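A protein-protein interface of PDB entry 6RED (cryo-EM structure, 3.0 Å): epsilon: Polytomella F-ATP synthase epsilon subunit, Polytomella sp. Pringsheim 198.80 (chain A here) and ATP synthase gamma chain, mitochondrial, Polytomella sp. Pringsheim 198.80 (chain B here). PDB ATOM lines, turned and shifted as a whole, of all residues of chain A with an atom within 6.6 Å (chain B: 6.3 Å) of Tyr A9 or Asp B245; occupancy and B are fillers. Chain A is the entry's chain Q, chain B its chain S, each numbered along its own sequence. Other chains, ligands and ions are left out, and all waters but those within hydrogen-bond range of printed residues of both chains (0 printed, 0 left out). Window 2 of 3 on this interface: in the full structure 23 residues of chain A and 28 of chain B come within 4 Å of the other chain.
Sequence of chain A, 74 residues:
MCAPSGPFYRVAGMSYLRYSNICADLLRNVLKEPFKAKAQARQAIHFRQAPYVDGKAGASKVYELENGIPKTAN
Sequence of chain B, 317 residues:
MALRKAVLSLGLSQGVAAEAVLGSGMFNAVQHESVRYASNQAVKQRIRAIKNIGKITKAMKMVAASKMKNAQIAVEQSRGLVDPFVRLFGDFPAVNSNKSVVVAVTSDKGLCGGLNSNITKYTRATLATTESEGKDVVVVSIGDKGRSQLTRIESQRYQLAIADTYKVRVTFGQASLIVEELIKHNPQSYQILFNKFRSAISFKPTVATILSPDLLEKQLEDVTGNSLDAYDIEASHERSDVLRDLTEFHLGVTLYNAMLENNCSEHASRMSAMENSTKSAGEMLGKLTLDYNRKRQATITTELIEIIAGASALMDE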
ATOM      1  N   GLY A   6     -18.859 -10.126 -12.755  1.00  0.00           N
ATOM      2  CA  GLY A   6     -18.764 -11.563 -12.803  1.00  0.00           C
ATOM      3  C   GLY A   6     -17.352 -12.075 -12.619  1.00  0.00           C
ATOM      4  O   GLY A   6     -16.507 -11.418 -12.009  1.00  0.00           O
ATOM      5  N   PRO A   7     -17.073 -13.271 -13.150  1.00  0.00           N
ATOM      6  CA  PRO A   7     -15.720 -13.834 -13.057  1.00  0.00           C
ATOM      7  C   PRO A   7     -14.686 -13.076 -13.877  1.00  0.00           C
ATOM      8  O   PRO A   7     -15.024 -12.124 -14.583  1.00  0.00           O
ATOM      9  CB  PRO A   7     -15.910 -15.262 -13.573  1.00  0.00           C
ATOM     10  CG  PRO A   7     -17.349 -15.548 -13.346  1.00  0.00           C
ATOM     11  CD  PRO A   7     -18.045 -14.270 -13.617  1.00  0.00           C
ATOM     12  N   PHE A   8     -13.420 -13.493 -13.786  1.00  0.00           N
ATOM     13  CA  PHE A   8     -12.329 -12.674 -14.304  1.00  0.00           C
ATOM     14  C   PHE A   8     -12.307 -12.631 -15.821  1.00  0.00           C
ATOM     15  O   PHE A   8     -11.907 -11.617 -16.402  1.00  0.00           O
ATOM     16  CB  PHE A   8     -10.989 -13.172 -13.771  1.00  0.00           C
ATOM     17  CG  PHE A   8     -10.582 -14.534 -14.265  1.00  0.00           C
ATOM     18  CD1 PHE A   8      -9.715 -14.671 -15.334  1.00  0.00           C
ATOM     19  CD2 PHE A   8     -11.025 -15.676 -13.626  1.00  0.00           C
ATOM     20  CE1 PHE A   8      -9.330 -15.906 -15.773  1.00  0.00           C
ATOM     21  CE2 PHE A   8     -10.637 -16.917 -14.064  1.00  0.00           C
ATOM     22  CZ  PHE A   8      -9.787 -17.030 -15.138  1.00  0.00           C
ATOM     23  N   TYR A   9     -12.711 -13.713 -16.477  1.00  0.00           N
ATOM     24  CA  TYR A   9     -12.898 -13.661 -17.917  1.00  0.00           C
ATOM     25  C   TYR A   9     -14.083 -12.783 -18.275  1.00  0.00           C
ATOM     26  O   TYR A   9     -14.046 -12.077 -19.287  1.00  0.00           O
ATOM     27  CB  TYR A   9     -13.080 -15.070 -18.481  1.00  0.00           C
ATOM     28  CG  TYR A   9     -14.076 -15.938 -17.745  1.00  0.00           C
ATOM     29  CD1 TYR A   9     -13.666 -16.792 -16.739  1.00  0.00           C
ATOM     30  CD2 TYR A   9     -15.418 -15.925 -18.076  1.00  0.00           C
ATOM     31  CE1 TYR A   9     -14.564 -17.582 -16.074  1.00  0.00           C
ATOM     32  CE2 TYR A   9     -16.320 -16.711 -17.416  1.00  0.00           C
ATOM     33  CZ  TYR A   9     -15.888 -17.537 -16.420  1.00  0.00           C
ATOM     34  OH  TYR A   9     -16.790 -18.327 -15.762  1.00  0.00           O
ATOM     35  N   ARG A  10     -15.114 -12.779 -17.438  1.00  0.00           N
ATOM     36  CA  ARG A  10     -16.346 -12.094 -17.784  1.00  0.00           C
ATOM     37  C   ARG A  10     -16.199 -10.584 -17.671  1.00  0.00           C
ATOM     38  O   ARG A  10     -16.828  -9.845 -18.436  1.00  0.00           O
ATOM     39  CB  ARG A  10     -17.475 -12.603 -16.897  1.00  0.00           C
ATOM     40  CG  ARG A  10     -18.850 -12.188 -17.335  1.00  0.00           C
ATOM     41  CD  ARG A  10     -19.196 -12.783 -18.676  1.00  0.00           C
ATOM     42  NE  ARG A  10     -19.259 -14.236 -18.636  1.00  0.00           N
ATOM     43  CZ  ARG A  10     -19.872 -14.968 -19.555  1.00  0.00           C
ATOM     44  NH1 ARG A  10     -20.473 -14.381 -20.577  1.00  0.00           N
ATOM     45  NH2 ARG A  10     -19.889 -16.283 -19.449  1.00  0.00           N
ATOM     46  N   VAL A  11     -15.358 -10.103 -16.751  1.00  0.00           N
ATOM     47  CA  VAL A  11     -15.086  -8.668 -16.701  1.00  0.00           C
ATOM     48  C   VAL A  11     -14.144  -8.230 -17.806  1.00  0.00           C
ATOM     49  O   VAL A  11     -14.006  -7.024 -18.045  1.00  0.00           O
ATOM     50  CB  VAL A  11     -14.485  -8.208 -15.359  1.00  0.00           C
ATOM     51  CG1 VAL A  11     -15.385  -8.610 -14.208  1.00  0.00           C
ATOM     52  CG2 VAL A  11     -13.078  -8.735 -15.172  1.00  0.00           C
ATOM     53  N   ALA A  12     -13.491  -9.166 -18.481  1.00  0.00           N
ATOM     54  CA  ALA A  12     -12.654  -8.854 -19.625  1.00  0.00           C
ATOM     55  C   ALA A  12     -13.432  -8.859 -20.926  1.00  0.00           C
ATOM     56  O   ALA A  12     -12.853  -8.577 -21.976  1.00  0.00           O
ATOM     57  CB  ALA A  12     -11.492  -9.844 -19.718  1.00  0.00           C
ATOM     58  N   GLY A  13     -14.724  -9.171 -20.880  1.00  0.00           N
ATOM     59  CA  GLY A  13     -15.500  -9.403 -22.077  1.00  0.00           C
ATOM     60  C   GLY A  13     -15.363 -10.790 -22.659  1.00  0.00           C
ATOM     61  O   GLY A  13     -16.160 -11.160 -23.529  1.00  0.00           O
ATOM     62  N   MET A  14     -14.382 -11.563 -22.206  1.00  0.00           N
ATOM     63  CA  MET A  14     -14.187 -12.931 -22.653  1.00  0.00           C
ATOM     64  C   MET A  14     -15.339 -13.794 -22.163  1.00  0.00           C
ATOM     65  O   MET A  14     -15.659 -13.797 -20.974  1.00  0.00           O
ATOM     66  CB  MET A  14     -12.850 -13.453 -22.132  1.00  0.00           C
ATOM     67  CG  MET A  14     -12.544 -14.879 -22.474  1.00  0.00           C
ATOM     68  SD  MET A  14     -11.084 -15.486 -21.618  1.00  0.00           S
ATOM     69  CE  MET A  14      -9.787 -14.674 -22.522  1.00  0.00           C
ATOM     70  N   SER A  15     -15.975 -14.509 -23.085  1.00  0.00           N
ATOM     71  CA  SER A  15     -17.124 -15.336 -22.760  1.00  0.00           C
ATOM     72  C   SER A  15     -16.684 -16.574 -21.987  1.00  0.00           C
ATOM     73  O   SER A  15     -15.493 -16.836 -21.810  1.00  0.00           O
ATOM     74  CB  SER A  15     -17.852 -15.727 -24.037  1.00  0.00           C
ATOM     75  OG  SER A  15     -18.888 -16.637 -23.764  1.00  0.00           O
ATOM     76  N   TYR A  16     -17.657 -17.362 -21.518  1.00  0.00           N
ATOM     77  CA  TYR A  16     -17.281 -18.624 -20.897  1.00  0.00           C
ATOM     78  C   TYR A  16     -16.767 -19.604 -21.927  1.00  0.00           C
ATOM     79  O   TYR A  16     -15.869 -20.396 -21.629  1.00  0.00           O
ATOM     80  CB  TYR A  16     -18.435 -19.270 -20.139  1.00  0.00           C
ATOM     81  CG  TYR A  16     -17.956 -20.501 -19.406  1.00  0.00           C
ATOM     82  CD1 TYR A  16     -17.167 -20.385 -18.277  1.00  0.00           C
ATOM     83  CD2 TYR A  16     -18.242 -21.775 -19.871  1.00  0.00           C
ATOM     84  CE1 TYR A  16     -16.701 -21.497 -17.622  1.00  0.00           C
ATOM     85  CE2 TYR A  16     -17.771 -22.886 -19.225  1.00  0.00           C
ATOM     86  CZ  TYR A  16     -17.006 -22.741 -18.100  1.00  0.00           C
ATOM     87  OH  TYR A  16     -16.541 -23.850 -17.442  1.00  0.00           O
ATOM     88  N   LEU A  17     -17.324 -19.569 -23.134  1.00  0.00           N
ATOM     89  CA  LEU A  17     -16.921 -20.516 -24.160  1.00  0.00           C
ATOM     90  C   LEU A  17     -15.512 -20.233 -24.635  1.00  0.00           C
ATOM     91  O   LEU A  17     -14.715 -21.161 -24.809  1.00  0.00           O
ATOM     92  CB  LEU A  17     -17.900 -20.467 -25.322  1.00  0.00           C
ATOM     93  CG  LEU A  17     -19.147 -21.293 -25.078  1.00  0.00           C
ATOM     94  CD1 LEU A  17     -20.051 -21.182 -26.267  1.00  0.00           C
ATOM     95  CD2 LEU A  17     -18.753 -22.727 -24.837  1.00  0.00           C
ATOM     96  N   TYR A  19     -13.181 -18.675 -22.860  1.00  0.00           N
ATOM     97  CA  TYR A  19     -12.296 -18.980 -21.741  1.00  0.00           C
ATOM     98  C   TYR A  19     -12.053 -20.478 -21.611  1.00  0.00           C
ATOM     99  O   TYR A  19     -10.908 -20.926 -21.471  1.00  0.00           O
ATOM    100  CB  TYR A  19     -12.898 -18.427 -20.451  1.00  0.00           C
ATOM    101  CG  TYR A  19     -12.354 -19.074 -19.210  1.00  0.00           C
ATOM    102  CD1 TYR A  19     -13.128 -19.948 -18.466  1.00  0.00           C
ATOM    103  CD2 TYR A  19     -11.063 -18.809 -18.781  1.00  0.00           C
ATOM    104  CE1 TYR A  19     -12.630 -20.544 -17.343  1.00  0.00           C
ATOM    105  CE2 TYR A  19     -10.564 -19.394 -17.655  1.00  0.00           C
ATOM    106  CZ  TYR A  19     -11.348 -20.265 -16.941  1.00  0.00           C
ATOM    107  OH  TYR A  19     -10.849 -20.857 -15.810  1.00  0.00           O
ATOM    108  N   PRO B 213     -30.234 -17.176 -19.372  1.00  0.00           N
ATOM    109  CA  PRO B 213     -30.177 -17.404 -17.922  1.00  0.00           C
ATOM    110  C   PRO B 213     -31.042 -16.492 -17.072  1.00  0.00           C
ATOM    111  O   PRO B 213     -31.956 -16.963 -16.388  1.00  0.00           O
ATOM    112  CB  PRO B 213     -28.693 -17.187 -17.603  1.00  0.00           C
ATOM    113  CG  PRO B 213     -28.171 -16.392 -18.724  1.00  0.00           C
ATOM    114  CD  PRO B 213     -28.904 -16.867 -19.914  1.00  0.00           C
ATOM    115  N   SER B 236     -17.588 -19.432  -8.228  1.00  0.00           N
ATOM    116  CA  SER B 236     -16.952 -18.210  -7.750  1.00  0.00           C
ATOM    117  C   SER B 236     -17.978 -17.142  -7.412  1.00  0.00           C
ATOM    118  O   SER B 236     -18.067 -16.686  -6.268  1.00  0.00           O
ATOM    119  CB  SER B 236     -15.999 -17.680  -8.810  1.00  0.00           C
ATOM    120  OG  SER B 236     -16.739 -17.202  -9.914  1.00  0.00           O
ATOM    121  N   SER B 240     -26.398 -15.943 -11.084  1.00  0.00           N
ATOM    122  CA  SER B 240     -26.685 -15.278 -12.346  1.00  0.00           C
ATOM    123  C   SER B 240     -25.504 -15.319 -13.303  1.00  0.00           C
ATOM    124  O   SER B 240     -25.680 -15.029 -14.490  1.00  0.00           O
ATOM    125  CB  SER B 240     -27.085 -13.826 -12.110  1.00  0.00           C
ATOM    126  OG  SER B 240     -25.966 -13.056 -11.716  1.00  0.00           O
ATOM    127  N   ASP B 241     -24.308 -15.643 -12.820  1.00  0.00           N
ATOM    128  CA  ASP B 241     -23.178 -15.891 -13.697  1.00  0.00           C
ATOM    129  C   ASP B 241     -22.903 -17.367 -13.914  1.00  0.00           C
ATOM    130  O   ASP B 241     -22.424 -17.737 -14.989  1.00  0.00           O
ATOM    131  CB  ASP B 241     -21.925 -15.211 -13.151  1.00  0.00           C
ATOM    132  CG  ASP B 241     -21.886 -13.733 -13.477  1.00  0.00           C
ATOM    133  OD1 ASP B 241     -21.485 -13.388 -14.608  1.00  0.00           O
ATOM    134  OD2 ASP B 241     -22.264 -12.914 -12.611  1.00  0.00           O
ATOM    135  N   VAL B 242     -23.215 -18.218 -12.934  1.00  0.00           N
ATOM    136  CA  VAL B 242     -23.103 -19.661 -13.127  1.00  0.00           C
ATOM    137  C   VAL B 242     -24.081 -20.130 -14.183  1.00  0.00           C
ATOM    138  O   VAL B 242     -23.744 -20.949 -15.040  1.00  0.00           O
ATOM    139  CB  VAL B 242     -23.336 -20.397 -11.802  1.00  0.00           C
ATOM    140  CG1 VAL B 242     -22.972 -21.855 -11.937  1.00  0.00           C
ATOM    141  CG2 VAL B 242     -22.541 -19.740 -10.732  1.00  0.00           C
ATOM    142  N   LEU B 243     -25.296 -19.595 -14.158  1.00  0.00           N
ATOM    143  CA  LEU B 243     -26.273 -19.959 -15.169  1.00  0.00           C
ATOM    144  C   LEU B 243     -25.945 -19.330 -16.509  1.00  0.00           C
ATOM    145  O   LEU B 243     -26.266 -19.907 -17.546  1.00  0.00           O
ATOM    146  CB  LEU B 243     -27.665 -19.562 -14.713  1.00  0.00           C
ATOM    147  CG  LEU B 243     -28.513 -20.704 -14.167  1.00  0.00           C
ATOM    148  CD1 LEU B 243     -27.850 -21.426 -13.020  1.00  0.00           C
ATOM    149  CD2 LEU B 243     -29.833 -20.145 -13.727  1.00  0.00           C
ATOM    150  N   ARG B 244     -25.269 -18.183 -16.512  1.00  0.00           N
ATOM    151  CA  ARG B 244     -24.814 -17.600 -17.767  1.00  0.00           C
ATOM    152  C   ARG B 244     -23.773 -18.484 -18.432  1.00  0.00           C
ATOM    153  O   ARG B 244     -23.890 -18.810 -19.620  1.00  0.00           O
ATOM    154  CB  ARG B 244     -24.246 -16.211 -17.524  1.00  0.00           C
ATOM    155  CG  ARG B 244     -23.726 -15.558 -18.774  1.00  0.00           C
ATOM    156  CD  ARG B 244     -23.213 -14.164 -18.490  1.00  0.00           C
ATOM    157  NE  ARG B 244     -24.018 -13.480 -17.483  1.00  0.00           N
ATOM    158  CZ  ARG B 244     -25.133 -12.807 -17.745  1.00  0.00           C
ATOM    159  NH1 ARG B 244     -25.799 -12.218 -16.764  1.00  0.00           N
ATOM    160  NH2 ARG B 244     -25.585 -12.733 -18.990  1.00  0.00           N
ATOM    161  N   ASP B 245     -22.766 -18.901 -17.663  1.00  0.00           N
ATOM    162  CA  ASP B 245     -21.737 -19.800 -18.169  1.00  0.00           C
ATOM    163  C   ASP B 245     -22.326 -21.138 -18.575  1.00  0.00           C
ATOM    164  O   ASP B 245     -21.933 -21.712 -19.595  1.00  0.00           O
ATOM    165  CB  ASP B 245     -20.668 -20.011 -17.106  1.00  0.00           C
ATOM    166  CG  ASP B 245     -19.998 -18.728 -16.695  1.00  0.00           C
ATOM    167  OD1 ASP B 245     -19.988 -17.775 -17.499  1.00  0.00           O
ATOM    168  OD2 ASP B 245     -19.479 -18.676 -15.562  1.00  0.00           O
ATOM    169  N   LEU B 246     -23.313 -21.618 -17.825  1.00  0.00           N
ATOM    170  CA  LEU B 246     -23.894 -22.916 -18.118  1.00  0.00           C
ATOM    171  C   LEU B 246     -24.756 -22.884 -19.370  1.00  0.00           C
ATOM    172  O   LEU B 246     -24.739 -23.835 -20.147  1.00  0.00           O
ATOM    173  CB  LEU B 246     -24.705 -23.399 -16.926  1.00  0.00           C
ATOM    174  CG  LEU B 246     -24.024 -24.368 -15.980  1.00  0.00           C
ATOM    175  CD1 LEU B 246     -25.049 -24.930 -15.053  1.00  0.00           C
ATOM    176  CD2 LEU B 246     -23.365 -25.469 -16.751  1.00  0.00           C
ATOM    177  N   THR B 247     -25.501 -21.808 -19.608  1.00  0.00           N
ATOM    178  CA  THR B 247     -26.291 -21.784 -20.833  1.00  0.00           C
ATOM    179  C   THR B 247     -25.466 -21.427 -22.058  1.00  0.00           C
ATOM    180  O   THR B 247     -25.817 -21.855 -23.159  1.00  0.00           O
ATOM    181  CB  THR B 247     -27.472 -20.835 -20.719  1.00  0.00           C
ATOM    182  OG1 THR B 247     -26.996 -19.498 -20.555  1.00  0.00           O
ATOM    183  CG2 THR B 247     -28.382 -21.246 -19.591  1.00  0.00           C
ATOM    184  N   GLU B 248     -24.367 -20.685 -21.907  1.00  0.00           N
ATOM    185  CA  GLU B 248     -23.454 -20.530 -23.036  1.00  0.00           C
ATOM    186  C   GLU B 248     -22.787 -21.854 -23.384  1.00  0.00           C
ATOM    187  O   GLU B 248     -22.695 -22.219 -24.564  1.00  0.00           O
ATOM    188  CB  GLU B 248     -22.418 -19.463 -22.724  1.00  0.00           C
ATOM    189  CG  GLU B 248     -23.020 -18.075 -22.648  1.00  0.00           C
ATOM    190  CD  GLU B 248     -22.018 -16.976 -22.893  1.00  0.00           C
ATOM    191  OE1 GLU B 248     -21.050 -17.222 -23.634  1.00  0.00           O
ATOM    192  OE2 GLU B 248     -22.202 -15.865 -22.356  1.00  0.00           O
ATOM    193  N   PHE B 249     -22.364 -22.604 -22.368  1.00  0.00           N
ATOM    194  CA  PHE B 249     -21.852 -23.950 -22.566  1.00  0.00           C
ATOM    195  C   PHE B 249     -22.895 -24.864 -23.177  1.00  0.00           C
ATOM    196  O   PHE B 249     -22.569 -25.672 -24.043  1.00  0.00           O
ATOM    197  CB  PHE B 249     -21.383 -24.495 -21.221  1.00  0.00           C
ATOM    198  CG  PHE B 249     -20.527 -25.714 -21.305  1.00  0.00           C
ATOM    199  CD1 PHE B 249     -19.836 -26.034 -22.448  1.00  0.00           C
ATOM    200  CD2 PHE B 249     -20.393 -26.529 -20.208  1.00  0.00           C
ATOM    201  CE1 PHE B 249     -19.056 -27.154 -22.498  1.00  0.00           C
ATOM    202  CE2 PHE B 249     -19.616 -27.648 -20.257  1.00  0.00           C
ATOM    203  CZ  PHE B 249     -18.948 -27.961 -21.403  1.00  0.00           C
ATOM    204  N   HIS B 250     -24.152 -24.727 -22.769  1.00  0.00           N
ATOM    205  CA  HIS B 250     -25.191 -25.634 -23.237  1.00  0.00           C
ATOM    206  C   HIS B 250     -25.572 -25.333 -24.673  1.00  0.00           C
ATOM    207  O   HIS B 250     -25.831 -26.254 -25.453  1.00  0.00           O
ATOM    208  CB  HIS B 250     -26.393 -25.539 -22.306  1.00  0.00           C
ATOM    209  CG  HIS B 250     -27.572 -26.336 -22.749  1.00  0.00           C
ATOM    210  ND1 HIS B 250     -27.455 -27.578 -23.326  1.00  0.00           N
ATOM    211  CD2 HIS B 250     -28.897 -26.103 -22.622  1.00  0.00           C
ATOM    212  CE1 HIS B 250     -28.658 -28.058 -23.575  1.00  0.00           C
ATOM    213  NE2 HIS B 250     -29.551 -27.183 -23.154  1.00  0.00           N
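The side-chain hydroxyl of Tyr A9 lies within hydrogen-bond range of the side-chain carboxylate of Asp B245 (2.7 Å). The guanidinium group (NH2) of Arg A10 is in salt-bridge range of the side-chain carboxylate (OD1) of Asp B245, 2.5 Å away. NH1 of Arg A10 lies within salt-bridge range of OE2 of Glu B248 (2.9 Å). OE1 of Glu B248 sits close to OG of Ser A15 (2.2 Å).
The backbone carbonyl oxygen of Tyr A9 is in hydrogen-bond range of the backbone NH of Met A14 (3.0 Å). The backbone NH (N) of Leu A17 lies close to the side-chain hydroxyl (OG) of Ser A15. OD1 of Asp B241 lies within salt-bridge range of NE of Arg B244 (3.8 Å). The side-chain hydroxyl (OG1) of Thr B247 is in hydrogen-bond range of the backbone carbonyl oxygen (O) of Arg B244 (3.3 Å).
Gly A6 touches Asp B241 (CA to OD1, 3.7 Å). CG of Pro A7 touches OG of Ser B236, at 3.9 Å. OD1 of Asp B241 touches CD of Pro A7 (3.7 Å). Arg A10 touches Asp B241. CD of Arg B244 touches NH1 of Arg A10, at 3.5 Å. Tyr A16 touches Asp B245 (CB to OD1, 3.4 Å). CD1 of Leu A17 touches O of Glu B248, at 3.3 Å.
Printed residues of chain B within 4 Å of Pro A7: Ser B236 (3.9 Å) and Asp B241 (3.7 Å). Of the printed residues of chain B, Tyr A9 touches Asp B245. Printed residues of chain B within 4 Å of Arg A10: Asp B241, Arg B244, Asp B245 and Glu B248. Of the printed residues of chain B, Ser A15 touches Glu B248 (2.2 Å). Printed residues of chain A within 4 Å of Ser B236: Pro A7 (3.9 Å). Printed residues of chain A within 4 Å of Asp B241: Gly A6 (3.7 Å), Pro A7 (3.7 Å) and Arg A10 (3.98 Å). Of chain A, only Tyr A9 (2.7 Å), Arg A10 (2.5 Å) and Tyr A16 (3.4 Å) come within 4 Å of Asp B245.
Of the 13 printed residues of chain A, 7 touch a printed residue of chain B. Hydrophobic or aromatic side chains of chain A that line the printed part of chain B: Pro A7, Tyr A9, Tyr A16 and Leu A17. Along chain A the printed residues that touch a printed residue of chain B span positions 6 to 17. Of the 13 printed residues of chain B, 5 touch a printed residue of chain A. Among the printed residues, Asp or Glu carboxylates within 4 Å of a Lys or Arg side-chain nitrogen of the other chain: Arg A10 with Asp B245 and Arg A10 with Glu B248.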
